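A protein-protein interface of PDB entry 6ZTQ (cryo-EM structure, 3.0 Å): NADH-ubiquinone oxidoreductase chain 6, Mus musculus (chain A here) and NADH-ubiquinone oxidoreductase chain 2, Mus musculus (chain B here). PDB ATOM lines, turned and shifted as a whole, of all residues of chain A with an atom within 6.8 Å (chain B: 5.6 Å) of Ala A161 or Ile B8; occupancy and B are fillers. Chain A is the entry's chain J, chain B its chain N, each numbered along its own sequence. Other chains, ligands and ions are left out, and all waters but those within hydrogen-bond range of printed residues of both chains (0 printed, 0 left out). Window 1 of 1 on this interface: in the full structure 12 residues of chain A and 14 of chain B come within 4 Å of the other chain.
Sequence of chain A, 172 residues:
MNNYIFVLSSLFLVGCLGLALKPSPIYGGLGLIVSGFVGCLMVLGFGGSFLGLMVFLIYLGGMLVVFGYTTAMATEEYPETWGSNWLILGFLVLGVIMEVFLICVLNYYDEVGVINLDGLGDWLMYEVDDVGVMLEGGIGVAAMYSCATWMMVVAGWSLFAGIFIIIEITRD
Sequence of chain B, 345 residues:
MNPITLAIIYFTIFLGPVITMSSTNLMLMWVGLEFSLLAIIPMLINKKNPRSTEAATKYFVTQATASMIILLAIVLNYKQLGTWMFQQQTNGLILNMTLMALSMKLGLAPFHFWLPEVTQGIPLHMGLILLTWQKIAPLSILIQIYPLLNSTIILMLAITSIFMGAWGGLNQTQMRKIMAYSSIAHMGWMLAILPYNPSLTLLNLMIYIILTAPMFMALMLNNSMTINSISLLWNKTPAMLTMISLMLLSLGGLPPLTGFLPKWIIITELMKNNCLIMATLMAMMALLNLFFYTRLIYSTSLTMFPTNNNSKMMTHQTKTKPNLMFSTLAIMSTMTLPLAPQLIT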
ATOM      1  N   GLY A 156      -2.682   3.391 -25.948  1.00  0.00           N
ATOM      2  CA  GLY A 156      -3.330   2.173 -25.508  1.00  0.00           C
ATOM      3  C   GLY A 156      -2.578   1.489 -24.390  1.00  0.00           C
ATOM      4  O   GLY A 156      -3.184   0.936 -23.470  1.00  0.00           O
ATOM      5  N   TRP A 157      -1.250   1.534 -24.440  1.00  0.00           N
ATOM      6  CA  TRP A 157      -0.473   0.976 -23.344  1.00  0.00           C
ATOM      7  C   TRP A 157      -0.666   1.781 -22.075  1.00  0.00           C
ATOM      8  O   TRP A 157      -0.729   1.210 -20.983  1.00  0.00           O
ATOM      9  CB  TRP A 157       1.005   0.913 -23.697  1.00  0.00           C
ATOM     10  CG  TRP A 157       1.741   0.066 -22.746  1.00  0.00           C
ATOM     11  CD1 TRP A 157       2.440   0.479 -21.666  1.00  0.00           C
ATOM     12  CD2 TRP A 157       1.826  -1.357 -22.762  1.00  0.00           C
ATOM     13  NE1 TRP A 157       2.970  -0.593 -21.007  1.00  0.00           N
ATOM     14  CE2 TRP A 157       2.605  -1.737 -21.661  1.00  0.00           C
ATOM     15  CE3 TRP A 157       1.321  -2.347 -23.604  1.00  0.00           C
ATOM     16  CZ2 TRP A 157       2.895  -3.060 -21.379  1.00  0.00           C
ATOM     17  CZ3 TRP A 157       1.610  -3.657 -23.325  1.00  0.00           C
ATOM     18  CH2 TRP A 157       2.389  -4.004 -22.220  1.00  0.00           C
ATOM     19  N   SER A 158      -0.743   3.106 -22.194  1.00  0.00           N
ATOM     20  CA  SER A 158      -1.002   3.930 -21.021  1.00  0.00           C
ATOM     21  C   SER A 158      -2.293   3.515 -20.343  1.00  0.00           C
ATOM     22  O   SER A 158      -2.324   3.289 -19.131  1.00  0.00           O
ATOM     23  CB  SER A 158      -1.067   5.395 -21.416  1.00  0.00           C
ATOM     24  OG  SER A 158      -1.536   6.181 -20.342  1.00  0.00           O
ATOM     25  N   LEU A 159      -3.358   3.364 -21.121  1.00  0.00           N
ATOM     26  CA  LEU A 159      -4.643   2.976 -20.546  1.00  0.00           C
ATOM     27  C   LEU A 159      -4.584   1.576 -19.944  1.00  0.00           C
ATOM     28  O   LEU A 159      -5.007   1.351 -18.795  1.00  0.00           O
ATOM     29  CB  LEU A 159      -5.721   3.050 -21.619  1.00  0.00           C
ATOM     30  CG  LEU A 159      -5.861   4.368 -22.370  1.00  0.00           C
ATOM     31  CD1 LEU A 159      -6.883   4.251 -23.451  1.00  0.00           C
ATOM     32  CD2 LEU A 159      -6.220   5.487 -21.438  1.00  0.00           C
ATOM     33  N   PHE A 160      -4.080   0.619 -20.722  1.00  0.00           N
ATOM     34  CA  PHE A 160      -3.993  -0.765 -20.284  1.00  0.00           C
ATOM     35  C   PHE A 160      -3.228  -0.881 -18.976  1.00  0.00           C
ATOM     36  O   PHE A 160      -3.738  -1.413 -17.986  1.00  0.00           O
ATOM     37  CB  PHE A 160      -3.319  -1.590 -21.378  1.00  0.00           C
ATOM     38  CG  PHE A 160      -3.370  -3.072 -21.161  1.00  0.00           C
ATOM     39  CD1 PHE A 160      -4.538  -3.706 -20.795  1.00  0.00           C
ATOM     40  CD2 PHE A 160      -2.242  -3.836 -21.351  1.00  0.00           C
ATOM     41  CE1 PHE A 160      -4.571  -5.058 -20.605  1.00  0.00           C
ATOM     42  CE2 PHE A 160      -2.275  -5.188 -21.160  1.00  0.00           C
ATOM     43  CZ  PHE A 160      -3.441  -5.801 -20.791  1.00  0.00           C
ATOM     44  N   ALA A 161      -2.001  -0.372 -18.949  1.00  0.00           N
ATOM     45  CA  ALA A 161      -1.208  -0.428 -17.735  1.00  0.00           C
ATOM     46  C   ALA A 161      -1.817   0.396 -16.613  1.00  0.00           C
ATOM     47  O   ALA A 161      -1.616   0.078 -15.436  1.00  0.00           O
ATOM     48  CB  ALA A 161       0.202   0.047 -18.029  1.00  0.00           C
ATOM     49  N   GLY A 162      -2.554   1.456 -16.945  1.00  0.00           N
ATOM     50  CA  GLY A 162      -3.221   2.223 -15.918  1.00  0.00           C
ATOM     51  C   GLY A 162      -4.245   1.408 -15.173  1.00  0.00           C
ATOM     52  O   GLY A 162      -4.464   1.623 -13.984  1.00  0.00           O
ATOM     53  N   ILE A 163      -4.881   0.465 -15.858  1.00  0.00           N
ATOM     54  CA  ILE A 163      -5.830  -0.418 -15.182  1.00  0.00           C
ATOM     55  C   ILE A 163      -5.128  -1.216 -14.083  1.00  0.00           C
ATOM     56  O   ILE A 163      -5.596  -1.289 -12.936  1.00  0.00           O
ATOM     57  CB  ILE A 163      -6.519  -1.336 -16.204  1.00  0.00           C
ATOM     58  CG1 ILE A 163      -7.414  -0.516 -17.132  1.00  0.00           C
ATOM     59  CG2 ILE A 163      -7.322  -2.377 -15.498  1.00  0.00           C
ATOM     60  CD1 ILE A 163      -7.799  -1.211 -18.392  1.00  0.00           C
ATOM     61  N   PHE A 164      -3.991  -1.823 -14.422  1.00  0.00           N
ATOM     62  CA  PHE A 164      -3.218  -2.584 -13.447  1.00  0.00           C
ATOM     63  C   PHE A 164      -2.746  -1.691 -12.310  1.00  0.00           C
ATOM     64  O   PHE A 164      -2.774  -2.084 -11.136  1.00  0.00           O
ATOM     65  CB  PHE A 164      -2.020  -3.227 -14.137  1.00  0.00           C
ATOM     66  CG  PHE A 164      -2.379  -4.290 -15.133  1.00  0.00           C
ATOM     67  CD1 PHE A 164      -2.264  -5.619 -14.811  1.00  0.00           C
ATOM     68  CD2 PHE A 164      -2.807  -3.959 -16.398  1.00  0.00           C
ATOM     69  CE1 PHE A 164      -2.588  -6.589 -15.724  1.00  0.00           C
ATOM     70  CE2 PHE A 164      -3.130  -4.923 -17.307  1.00  0.00           C
ATOM     71  CZ  PHE A 164      -3.020  -6.240 -16.968  1.00  0.00           C
ATOM     72  N   ILE A 165      -2.297  -0.486 -12.652  1.00  0.00           N
ATOM     73  CA  ILE A 165      -1.844   0.480 -11.660  1.00  0.00           C
ATOM     74  C   ILE A 165      -2.967   0.830 -10.694  1.00  0.00           C
ATOM     75  O   ILE A 165      -2.756   0.929  -9.480  1.00  0.00           O
ATOM     76  CB  ILE A 165      -1.295   1.721 -12.382  1.00  0.00           C
ATOM     77  CG1 ILE A 165       0.052   1.402 -13.020  1.00  0.00           C
ATOM     78  CG2 ILE A 165      -1.163   2.889 -11.455  1.00  0.00           C
ATOM     79  CD1 ILE A 165       0.364   2.219 -14.213  1.00  0.00           C
ATOM     80  N   ILE A 166      -4.169   1.050 -11.226  1.00  0.00           N
ATOM     81  CA  ILE A 166      -5.340   1.339 -10.404  1.00  0.00           C
ATOM     82  C   ILE A 166      -5.572   0.214  -9.417  1.00  0.00           C
ATOM     83  O   ILE A 166      -5.739   0.439  -8.211  1.00  0.00           O
ATOM     84  CB  ILE A 166      -6.567   1.545 -11.307  1.00  0.00           C
ATOM     85  CG1 ILE A 166      -6.501   2.902 -11.980  1.00  0.00           C
ATOM     86  CG2 ILE A 166      -7.878   1.405 -10.545  1.00  0.00           C
ATOM     87  CD1 ILE A 166      -7.196   2.896 -13.302  1.00  0.00           C
ATOM     88  N   PRO B   3       2.440 -12.028 -11.159  1.00  0.00           N
ATOM     89  CA  PRO B   3       3.529 -11.813 -12.124  1.00  0.00           C
ATOM     90  C   PRO B   3       3.140 -10.983 -13.329  1.00  0.00           C
ATOM     91  O   PRO B   3       3.983 -10.244 -13.852  1.00  0.00           O
ATOM     92  CB  PRO B   3       3.910 -13.242 -12.532  1.00  0.00           C
ATOM     93  CG  PRO B   3       3.341 -14.102 -11.488  1.00  0.00           C
ATOM     94  CD  PRO B   3       2.082 -13.453 -11.114  1.00  0.00           C
ATOM     95  N   ILE B   4       1.905 -11.119 -13.815  1.00  0.00           N
ATOM     96  CA  ILE B   4       1.454 -10.323 -14.952  1.00  0.00           C
ATOM     97  C   ILE B   4       1.613  -8.843 -14.645  1.00  0.00           C
ATOM     98  O   ILE B   4       2.081  -8.054 -15.479  1.00  0.00           O
ATOM     99  CB  ILE B   4      -0.006 -10.675 -15.293  1.00  0.00           C
ATOM    100  CG1 ILE B   4      -0.105 -12.099 -15.847  1.00  0.00           C
ATOM    101  CG2 ILE B   4      -0.574  -9.689 -16.286  1.00  0.00           C
ATOM    102  CD1 ILE B   4      -1.496 -12.686 -15.793  1.00  0.00           C
ATOM    103  N   THR B   5       1.258  -8.456 -13.426  1.00  0.00           N
ATOM    104  CA  THR B   5       1.311  -7.058 -13.043  1.00  0.00           C
ATOM    105  C   THR B   5       2.747  -6.563 -12.973  1.00  0.00           C
ATOM    106  O   THR B   5       3.047  -5.444 -13.402  1.00  0.00           O
ATOM    107  CB  THR B   5       0.620  -6.885 -11.701  1.00  0.00           C
ATOM    108  OG1 THR B   5      -0.684  -7.464 -11.760  1.00  0.00           O
ATOM    109  CG2 THR B   5       0.483  -5.440 -11.368  1.00  0.00           C
ATOM    110  N   LEU B   6       3.643  -7.382 -12.427  1.00  0.00           N
ATOM    111  CA  LEU B   6       5.044  -6.996 -12.352  1.00  0.00           C
ATOM    112  C   LEU B   6       5.644  -6.853 -13.738  1.00  0.00           C
ATOM    113  O   LEU B   6       6.413  -5.921 -13.996  1.00  0.00           O
ATOM    114  CB  LEU B   6       5.828  -8.020 -11.544  1.00  0.00           C
ATOM    115  CG  LEU B   6       5.558  -8.025 -10.049  1.00  0.00           C
ATOM    116  CD1 LEU B   6       5.728  -9.403  -9.496  1.00  0.00           C
ATOM    117  CD2 LEU B   6       6.497  -7.077  -9.370  1.00  0.00           C
ATOM    118  N   ALA B   7       5.311  -7.774 -14.638  1.00  0.00           N
ATOM    119  CA  ALA B   7       5.764  -7.663 -16.019  1.00  0.00           C
ATOM    120  C   ALA B   7       5.322  -6.344 -16.629  1.00  0.00           C
ATOM    121  O   ALA B   7       6.133  -5.603 -17.194  1.00  0.00           O
ATOM    122  CB  ALA B   7       5.232  -8.835 -16.837  1.00  0.00           C
ATOM    123  N   ILE B   8       4.036  -6.025 -16.487  1.00  0.00           N
ATOM    124  CA  ILE B   8       3.492  -4.799 -17.064  1.00  0.00           C
ATOM    125  C   ILE B   8       4.201  -3.580 -16.489  1.00  0.00           C
ATOM    126  O   ILE B   8       4.645  -2.685 -17.221  1.00  0.00           O
ATOM    127  CB  ILE B   8       1.976  -4.735 -16.814  1.00  0.00           C
ATOM    128  CG1 ILE B   8       1.255  -5.863 -17.558  1.00  0.00           C
ATOM    129  CG2 ILE B   8       1.423  -3.370 -17.183  1.00  0.00           C
ATOM    130  CD1 ILE B   8       0.952  -5.571 -18.974  1.00  0.00           C
ATOM    131  N   ILE B   9       4.338  -3.540 -15.168  1.00  0.00           N
ATOM    132  CA  ILE B   9       4.838  -2.347 -14.500  1.00  0.00           C
ATOM    133  C   ILE B   9       6.318  -2.142 -14.792  1.00  0.00           C
ATOM    134  O   ILE B   9       6.761  -1.016 -15.054  1.00  0.00           O
ATOM    135  CB  ILE B   9       4.534  -2.443 -12.995  1.00  0.00           C
ATOM    136  CG1 ILE B   9       3.100  -1.994 -12.768  1.00  0.00           C
ATOM    137  CG2 ILE B   9       5.470  -1.603 -12.160  1.00  0.00           C
ATOM    138  CD1 ILE B   9       2.495  -2.446 -11.490  1.00  0.00           C
ATOM    139  N   TYR B  10       7.108  -3.212 -14.769  1.00  0.00           N
ATOM    140  CA  TYR B  10       8.528  -3.053 -15.026  1.00  0.00           C
ATOM    141  C   TYR B  10       8.799  -2.786 -16.497  1.00  0.00           C
ATOM    142  O   TYR B  10       9.723  -2.034 -16.824  1.00  0.00           O
ATOM    143  CB  TYR B  10       9.286  -4.283 -14.540  1.00  0.00           C
ATOM    144  CG  TYR B  10       9.658  -4.205 -13.080  1.00  0.00           C
ATOM    145  CD1 TYR B  10      10.637  -3.333 -12.638  1.00  0.00           C
ATOM    146  CD2 TYR B  10       9.023  -4.993 -12.146  1.00  0.00           C
ATOM    147  CE1 TYR B  10      10.970  -3.253 -11.312  1.00  0.00           C
ATOM    148  CE2 TYR B  10       9.348  -4.924 -10.818  1.00  0.00           C
ATOM    149  CZ  TYR B  10      10.324  -4.052 -10.404  1.00  0.00           C
ATOM    150  OH  TYR B  10      10.655  -3.977  -9.073  1.00  0.00           O
ATOM    151  N   PHE B  11       7.995  -3.356 -17.393  1.00  0.00           N
ATOM    152  CA  PHE B  11       8.077  -2.983 -18.795  1.00  0.00           C
ATOM    153  C   PHE B  11       7.803  -1.502 -18.981  1.00  0.00           C
ATOM    154  O   PHE B  11       8.506  -0.823 -19.735  1.00  0.00           O
ATOM    155  CB  PHE B  11       7.087  -3.808 -19.597  1.00  0.00           C
ATOM    156  CG  PHE B  11       7.240  -3.680 -21.072  1.00  0.00           C
ATOM    157  CD1 PHE B  11       8.191  -4.413 -21.740  1.00  0.00           C
ATOM    158  CD2 PHE B  11       6.416  -2.847 -21.796  1.00  0.00           C
ATOM    159  CE1 PHE B  11       8.328  -4.308 -23.099  1.00  0.00           C
ATOM    160  CE2 PHE B  11       6.547  -2.739 -23.155  1.00  0.00           C
ATOM    161  CZ  PHE B  11       7.501  -3.472 -23.809  1.00  0.00           C
ATOM    162  N   THR B  12       6.789  -0.982 -18.296  1.00  0.00           N
ATOM    163  CA  THR B  12       6.466   0.434 -18.413  1.00  0.00           C
ATOM    164  C   THR B  12       7.594   1.306 -17.875  1.00  0.00           C
ATOM    165  O   THR B  12       7.935   2.337 -18.470  1.00  0.00           O
ATOM    166  CB  THR B  12       5.163   0.707 -17.676  1.00  0.00           C
ATOM    167  OG1 THR B  12       4.161  -0.202 -18.134  1.00  0.00           O
ATOM    168  CG2 THR B  12       4.699   2.102 -17.912  1.00  0.00           C
ATOM    169  N   ILE B  13       8.185   0.905 -16.748  1.00  0.00           N
ATOM    170  CA  ILE B  13       9.295   1.662 -16.177  1.00  0.00           C
ATOM    171  C   ILE B  13      10.477   1.664 -17.131  1.00  0.00           C
ATOM    172  O   ILE B  13      11.163   2.679 -17.293  1.00  0.00           O
ATOM    173  CB  ILE B  13       9.684   1.089 -14.803  1.00  0.00           C
ATOM    174  CG1 ILE B  13       8.644   1.465 -13.772  1.00  0.00           C
ATOM    175  CG2 ILE B  13      11.007   1.630 -14.335  1.00  0.00           C
ATOM    176  CD1 ILE B  13       8.592   0.545 -12.637  1.00  0.00           C
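CH2 of Trp A157 touches CD1 of Ile B8, 3.9 Å away. Trp A157 touches Phe B11 (CZ2 to CD2, 3.6 Å). Ile B8 touches Phe A160 (CD1 to CE2, 3.9 Å). CB of Ala A161 touches CG2 of Ile B8, 3.7 Å away. Thr B12 touches Ala A161. Phe A164 touches Ile B4 (CE1 to CG2, 3.7 Å). Phe A164 touches Thr B5.
Printed residues of chain B within 4 Å of Trp A157: Ile B8, Phe B11 and Thr B12. Printed residues of chain B within 4 Å of Phe A160: Ile B8 (3.9 Å). Ala A161 touches just these residues of chain B: Ile B8 (3.7 Å) and Thr B12 (3.97 Å). Of the printed residues of chain A, Ile B4 touches Phe A164. Of the printed residues of chain A, Thr B5 touches Phe A164. Ala B7 touches none of the printed residues of chain A. Of chain A, only Trp A157 (3.9 Å), Phe A160 (3.9 Å) and Ala A161 (3.7 Å) come within 4 Å of Ile B8. The nearest printed residue of chain B that does not touch Phe A160 is Ile B4 (6.6 Å).
The backbone carbonyl oxygen (O) of Ile B8 is in hydrogen-bond range of the side-chain hydroxyl (OG1) of Thr B12 (2.7 Å).
Printed residues of chain A that touch a printed residue of chain B: Trp A157, Phe A160, Ala A161 and Phe A164. Hydrophobic or aromatic side chains of chain A that line the printed part of chain B: Trp A157, Phe A160, Ala A161 and Phe A164. Of the 11 printed residues of chain B, 5 touch a printed residue of chain A. Hydrophobic or aromatic side chains of chain B that line the printed part of chain A: Ile B4, Ile B8 and Phe B11. Among the printed residues, 8 pairs touch across the chains. Among the printed residues, no Asp or Glu carboxylate lies within 4 Å of a Lys or Arg side-chain nitrogen of the other chain.
The indole nitrogen (NE1) of Trp A157 is in hydrogen-bond range of the side-chain hydroxyl (OG1) of Thr B12 (3.1 Å).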
